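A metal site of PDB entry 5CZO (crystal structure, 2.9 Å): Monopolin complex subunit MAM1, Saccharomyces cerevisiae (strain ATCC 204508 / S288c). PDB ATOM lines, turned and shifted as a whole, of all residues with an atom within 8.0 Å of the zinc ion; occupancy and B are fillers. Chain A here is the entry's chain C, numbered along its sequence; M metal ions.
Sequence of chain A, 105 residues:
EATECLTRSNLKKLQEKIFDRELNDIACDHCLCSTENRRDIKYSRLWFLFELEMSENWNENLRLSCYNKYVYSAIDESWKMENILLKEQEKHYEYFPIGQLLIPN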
ATOM      1  N   ILE A  26     -15.290  10.202 -21.546  1.00  0.00           N
ATOM      2  CA  ILE A  26     -15.931   9.402 -22.582  1.00  0.00           C
ATOM      3  C   ILE A  26     -15.755  10.101 -23.925  1.00  0.00           C
ATOM      4  O   ILE A  26     -16.564  10.956 -24.312  1.00  0.00           O
ATOM      5  CB  ILE A  26     -17.427   9.175 -22.286  1.00  0.00           C
ATOM      6  CG1 ILE A  26     -17.614   8.499 -20.927  1.00  0.00           C
ATOM      7  CG2 ILE A  26     -18.066   8.339 -23.379  1.00  0.00           C
ATOM      8  CD1 ILE A  26     -19.046   8.160 -20.604  1.00  0.00           C
ATOM      9  N   ALA A  27     -14.694   9.753 -24.643  1.00  0.00           N
ATOM     10  CA  ALA A  27     -14.356  10.413 -25.889  1.00  0.00           C
ATOM     11  C   ALA A  27     -14.745   9.582 -27.107  1.00  0.00           C
ATOM     12  O   ALA A  27     -13.996   8.723 -27.560  1.00  0.00           O
ATOM     13  CB  ALA A  27     -12.864  10.727 -25.933  1.00  0.00           C
ATOM     14  N   CYS A  28     -15.939   9.848 -27.640  1.00  0.00           N
ATOM     15  CA  CYS A  28     -16.388   9.230 -28.874  1.00  0.00           C
ATOM     16  C   CYS A  28     -17.350  10.157 -29.612  1.00  0.00           C
ATOM     17  O   CYS A  28     -17.916  11.072 -29.022  1.00  0.00           O
ATOM     18  CB  CYS A  28     -17.068   7.884 -28.585  1.00  0.00           C
ATOM     19  SG  CYS A  28     -18.559   8.021 -27.582  1.00  0.00           S
ATOM     20  N   ASP A  29     -17.517   9.921 -30.909  1.00  0.00           N
ATOM     21  CA  ASP A  29     -18.376  10.776 -31.723  1.00  0.00           C
ATOM     22  C   ASP A  29     -19.812  10.252 -31.734  1.00  0.00           C
ATOM     23  O   ASP A  29     -20.649  10.716 -32.515  1.00  0.00           O
ATOM     24  CB  ASP A  29     -17.838  10.874 -33.148  1.00  0.00           C
ATOM     25  CG  ASP A  29     -18.355  12.103 -33.878  1.00  0.00           C
ATOM     26  OD1 ASP A  29     -18.857  13.023 -33.204  1.00  0.00           O
ATOM     27  OD2 ASP A  29     -18.243  12.150 -35.126  1.00  0.00           O
ATOM     28  N   HIS A  30     -20.097   9.290 -30.854  1.00  0.00           N
ATOM     29  CA  HIS A  30     -21.445   8.770 -30.689  1.00  0.00           C
ATOM     30  C   HIS A  30     -22.355   9.841 -30.108  1.00  0.00           C
ATOM     31  O   HIS A  30     -21.970  10.552 -29.180  1.00  0.00           O
ATOM     32  CB  HIS A  30     -21.431   7.533 -29.790  1.00  0.00           C
ATOM     33  CG  HIS A  30     -20.608   6.391 -30.319  1.00  0.00           C
ATOM     34  ND1 HIS A  30     -20.126   5.382 -29.524  1.00  0.00           N
ATOM     35  CD2 HIS A  30     -20.188   6.119 -31.582  1.00  0.00           C
ATOM     36  CE1 HIS A  30     -19.437   4.527 -30.263  1.00  0.00           C
ATOM     37  NE2 HIS A  30     -19.459   4.953 -31.509  1.00  0.00           N
ATOM     38  N   CYS A  31     -23.554   9.964 -30.666  1.00  0.00           N
ATOM     39  CA  CYS A  31     -24.491  11.018 -30.267  1.00  0.00           C
ATOM     40  C   CYS A  31     -25.083  10.777 -28.880  1.00  0.00           C
ATOM     41  O   CYS A  31     -25.193  11.692 -28.067  1.00  0.00           O
ATOM     42  CB  CYS A  31     -25.616  11.149 -31.294  1.00  0.00           C
ATOM     43  SG  CYS A  31     -25.597   9.867 -32.587  1.00  0.00           S
ATOM     44  N   LEU A  32     -25.476   9.526 -28.612  1.00  0.00           N
ATOM     45  CA  LEU A  32     -26.104   9.174 -27.347  1.00  0.00           C
ATOM     46  C   LEU A  32     -25.131   9.278 -26.164  1.00  0.00           C
ATOM     47  O   LEU A  32     -25.526   9.652 -25.061  1.00  0.00           O
ATOM     48  CB  LEU A  32     -26.680   7.756 -27.417  1.00  0.00           C
ATOM     49  CG  LEU A  32     -27.832   7.540 -28.409  1.00  0.00           C
ATOM     50  CD1 LEU A  32     -28.286   6.095 -28.387  1.00  0.00           C
ATOM     51  CD2 LEU A  32     -28.989   8.474 -28.103  1.00  0.00           C
ATOM     52  N   CYS A  33     -23.872   8.958 -26.417  1.00  0.00           N
ATOM     53  CA  CYS A  33     -22.843   8.953 -25.380  1.00  0.00           C
ATOM     54  C   CYS A  33     -22.364  10.371 -25.065  1.00  0.00           C
ATOM     55  O   CYS A  33     -21.767  10.610 -24.022  1.00  0.00           O
ATOM     56  CB  CYS A  33     -21.645   8.095 -25.802  1.00  0.00           C
ATOM     57  SG  CYS A  33     -22.034   6.424 -26.387  1.00  0.00           S
ATOM     58  N   SER A  34     -22.652  11.299 -25.969  1.00  0.00           N
ATOM     59  CA  SER A  34     -22.180  12.676 -25.852  1.00  0.00           C
ATOM     60  C   SER A  34     -22.715  13.346 -24.589  1.00  0.00           C
ATOM     61  O   SER A  34     -23.779  13.009 -24.080  1.00  0.00           O
ATOM     62  CB  SER A  34     -22.580  13.485 -27.084  1.00  0.00           C
ATOM     63  OG  SER A  34     -22.098  14.820 -26.992  1.00  0.00           O
ATOM     64  N   ARG A  38     -26.709  14.044 -22.080  1.00  0.00           N
ATOM     65  CA  ARG A  38     -26.903  13.777 -20.664  1.00  0.00           C
ATOM     66  C   ARG A  38     -27.466  14.987 -19.934  1.00  0.00           C
ATOM     67  O   ARG A  38     -28.119  14.845 -18.894  1.00  0.00           O
ATOM     68  CB  ARG A  38     -25.593  13.335 -20.025  1.00  0.00           C
ATOM     69  CG  ARG A  38     -24.977  12.091 -20.667  1.00  0.00           C
ATOM     70  CD  ARG A  38     -23.630  11.765 -20.058  1.00  0.00           C
ATOM     71  NE  ARG A  38     -22.612  11.559 -21.076  1.00  0.00           N
ATOM     72  CZ  ARG A  38     -21.350  11.243 -20.806  1.00  0.00           C
ATOM     73  NH1 ARG A  38     -20.954  11.100 -19.554  1.00  0.00           N
ATOM     74  NH2 ARG A  38     -20.483  11.077 -21.798  1.00  0.00           N
ATOM     75  N   TRP A  47     -30.815   7.393 -19.544  1.00  0.00           N
ATOM     76  CA  TRP A  47     -29.648   7.407 -20.414  1.00  0.00           C
ATOM     77  C   TRP A  47     -28.812   6.147 -20.223  1.00  0.00           C
ATOM     78  O   TRP A  47     -28.522   5.430 -21.176  1.00  0.00           O
ATOM     79  CB  TRP A  47     -28.792   8.640 -20.144  1.00  0.00           C
ATOM     80  CG  TRP A  47     -27.495   8.630 -20.882  1.00  0.00           C
ATOM     81  CD1 TRP A  47     -27.297   8.938 -22.202  1.00  0.00           C
ATOM     82  CD2 TRP A  47     -26.203   8.298 -20.357  1.00  0.00           C
ATOM     83  NE1 TRP A  47     -25.965   8.809 -22.521  1.00  0.00           N
ATOM     84  CE2 TRP A  47     -25.269   8.416 -21.405  1.00  0.00           C
ATOM     85  CE3 TRP A  47     -25.748   7.903 -19.094  1.00  0.00           C
ATOM     86  CZ2 TRP A  47     -23.917   8.165 -21.236  1.00  0.00           C
ATOM     87  CZ3 TRP A  47     -24.397   7.642 -18.925  1.00  0.00           C
ATOM     88  CH2 TRP A  47     -23.502   7.780 -19.988  1.00  0.00           C
ATOM     89  N   LEU A  52     -28.352   3.591 -23.509  1.00  0.00           N
ATOM     90  CA  LEU A  52     -27.091   2.882 -23.731  1.00  0.00           C
ATOM     91  C   LEU A  52     -27.359   1.449 -24.191  1.00  0.00           C
ATOM     92  O   LEU A  52     -26.436   0.698 -24.493  1.00  0.00           O
ATOM     93  CB  LEU A  52     -26.228   2.888 -22.474  1.00  0.00           C
ATOM     94  CG  LEU A  52     -25.588   4.226 -22.079  1.00  0.00           C
ATOM     95  CD1 LEU A  52     -24.519   4.020 -21.018  1.00  0.00           C
ATOM     96  CD2 LEU A  52     -25.019   4.917 -23.304  1.00  0.00           C
ATOM     97  N   GLU A  56     -24.151   0.816 -31.628  1.00  0.00           N
ATOM     98  CA  GLU A  56     -23.598   1.612 -32.713  1.00  0.00           C
ATOM     99  C   GLU A  56     -22.927   0.726 -33.763  1.00  0.00           C
ATOM    100  O   GLU A  56     -22.887   1.075 -34.947  1.00  0.00           O
ATOM    101  CB  GLU A  56     -22.590   2.634 -32.179  1.00  0.00           C
ATOM    102  CG  GLU A  56     -22.312   3.792 -33.120  1.00  0.00           C
ATOM    103  CD  GLU A  56     -23.309   4.913 -32.974  1.00  0.00           C
ATOM    104  OE1 GLU A  56     -23.905   5.035 -31.879  1.00  0.00           O
ATOM    105  OE2 GLU A  56     -23.498   5.689 -33.936  1.00  0.00           O
ATOM    106  N   ASN A  61     -23.592  -3.189 -27.243  1.00  0.00           N
ATOM    107  CA  ASN A  61     -24.355  -1.984 -26.950  1.00  0.00           C
ATOM    108  C   ASN A  61     -23.419  -0.875 -26.480  1.00  0.00           C
ATOM    109  O   ASN A  61     -22.230  -1.113 -26.264  1.00  0.00           O
ATOM    110  CB  ASN A  61     -25.446  -2.264 -25.895  1.00  0.00           C
ATOM    111  CG  ASN A  61     -24.902  -2.885 -24.623  1.00  0.00           C
ATOM    112  OD1 ASN A  61     -23.756  -2.660 -24.237  1.00  0.00           O
ATOM    113  ND2 ASN A  61     -25.736  -3.681 -23.959  1.00  0.00           N
ATOM    114  N   LEU A  62     -23.950   0.335 -26.332  1.00  0.00           N
ATOM    115  CA  LEU A  62     -23.124   1.487 -25.986  1.00  0.00           C
ATOM    116  C   LEU A  62     -22.568   1.394 -24.567  1.00  0.00           C
ATOM    117  O   LEU A  62     -21.512   1.946 -24.273  1.00  0.00           O
ATOM    118  CB  LEU A  62     -23.930   2.777 -26.157  1.00  0.00           C
ATOM    119  CG  LEU A  62     -24.293   3.130 -27.600  1.00  0.00           C
ATOM    120  CD1 LEU A  62     -25.026   4.458 -27.660  1.00  0.00           C
ATOM    121  CD2 LEU A  62     -23.046   3.150 -28.465  1.00  0.00           C
ATOM    122  N   ARG A  63     -23.284   0.685 -23.684  1.00  0.00           N
ATOM    123  CA  ARG A  63     -22.827   0.533 -22.306  1.00  0.00           C
ATOM    124  C   ARG A  63     -21.607  -0.375 -22.228  1.00  0.00           C
ATOM    125  O   ARG A  63     -20.840  -0.325 -21.275  1.00  0.00           O
ATOM    126  CB  ARG A  63     -23.967  -0.005 -21.429  1.00  0.00           C
ATOM    127  CG  ARG A  63     -23.652   0.012 -19.938  1.00  0.00           C
ATOM    128  CD  ARG A  63     -24.919  -0.028 -19.082  1.00  0.00           C
ATOM    129  NE  ARG A  63     -25.637  -1.293 -19.197  1.00  0.00           N
ATOM    130  CZ  ARG A  63     -26.768  -1.458 -19.881  1.00  0.00           C
ATOM    131  NH1 ARG A  63     -27.301  -0.420 -20.511  1.00  0.00           N
ATOM    132  NH2 ARG A  63     -27.357  -2.641 -19.926  1.00  0.00           N
ATOM    133  N   SER A  65     -19.417  -0.988 -25.261  1.00  0.00           N
ATOM    134  CA  SER A  65     -18.369  -0.498 -26.159  1.00  0.00           C
ATOM    135  C   SER A  65     -17.820   0.857 -25.732  1.00  0.00           C
ATOM    136  O   SER A  65     -16.626   1.117 -25.860  1.00  0.00           O
ATOM    137  CB  SER A  65     -18.905  -0.428 -27.594  1.00  0.00           C
ATOM    138  OG  SER A  65     -19.972   0.510 -27.695  1.00  0.00           O
ATOM    139  N   CYS A  66     -18.702   1.727 -25.239  1.00  0.00           N
ATOM    140  CA  CYS A  66     -18.299   3.092 -24.883  1.00  0.00           C
ATOM    141  C   CYS A  66     -18.099   3.268 -23.376  1.00  0.00           C
ATOM    142  O   CYS A  66     -17.029   3.703 -22.937  1.00  0.00           O
ATOM    143  CB  CYS A  66     -19.335   4.099 -25.383  1.00  0.00           C
ATOM    144  SG  CYS A  66     -19.461   4.201 -27.186  1.00  0.00           S
ATOM    145  N   TYR A  67     -19.113   2.936 -22.593  1.00  0.00           N
ATOM    146  CA  TYR A  67     -19.055   3.192 -21.155  1.00  0.00           C
ATOM    147  C   TYR A  67     -18.039   2.307 -20.458  1.00  0.00           C
ATOM    148  O   TYR A  67     -17.200   2.797 -19.698  1.00  0.00           O
ATOM    149  CB  TYR A  67     -20.435   2.984 -20.511  1.00  0.00           C
ATOM    150  CG  TYR A  67     -20.554   3.653 -19.159  1.00  0.00           C
ATOM    151  CD1 TYR A  67     -20.133   3.006 -18.003  1.00  0.00           C
ATOM    152  CD2 TYR A  67     -21.070   4.928 -19.047  1.00  0.00           C
ATOM    153  CE1 TYR A  67     -20.236   3.622 -16.765  1.00  0.00           C
ATOM    154  CE2 TYR A  67     -21.173   5.553 -17.820  1.00  0.00           C
ATOM    155  CZ  TYR A  67     -20.760   4.894 -16.684  1.00  0.00           C
ATOM    156  OH  TYR A  67     -20.862   5.519 -15.457  1.00  0.00           O
ATOM    157  N   TYR A  70     -14.307   3.390 -21.339  1.00  0.00           N
ATOM    158  CA  TYR A  70     -13.812   4.689 -20.900  1.00  0.00           C
ATOM    159  C   TYR A  70     -13.952   4.902 -19.390  1.00  0.00           C
ATOM    160  O   TYR A  70     -13.115   5.579 -18.770  1.00  0.00           O
ATOM    161  CB  TYR A  70     -14.534   5.805 -21.652  1.00  0.00           C
ATOM    162  CG  TYR A  70     -14.276   5.811 -23.137  1.00  0.00           C
ATOM    163  CD1 TYR A  70     -13.042   5.425 -23.647  1.00  0.00           C
ATOM    164  CD2 TYR A  70     -15.259   6.199 -24.041  1.00  0.00           C
ATOM    165  CE1 TYR A  70     -12.793   5.423 -25.011  1.00  0.00           C
ATOM    166  CE2 TYR A  70     -15.030   6.199 -25.396  1.00  0.00           C
ATOM    167  CZ  TYR A  70     -13.788   5.816 -25.876  1.00  0.00           C
ATOM    168  OH  TYR A  70     -13.550   5.816 -27.231  1.00  0.00           O
HETATM  169 ZN    ZN M   1     -20.146   6.356 -27.703  1.00  0.00          ZN
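The zinc ion is bound by ND1 of His 30, SG of Cys 33, SG of Cys 28 and SG of Cys 66. The zinc ion has four donor atoms within binding distance.
The guanidinium group (NH2) of Arg 38 is in hydrogen-bond range of the backbone carbonyl oxygen (O) of Cys 33 (2.6 Å). The side-chain sulfur (SG) of Cys 66 sits close to the side-chain hydroxyl (OG) of Ser 65 (3.8 Å).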
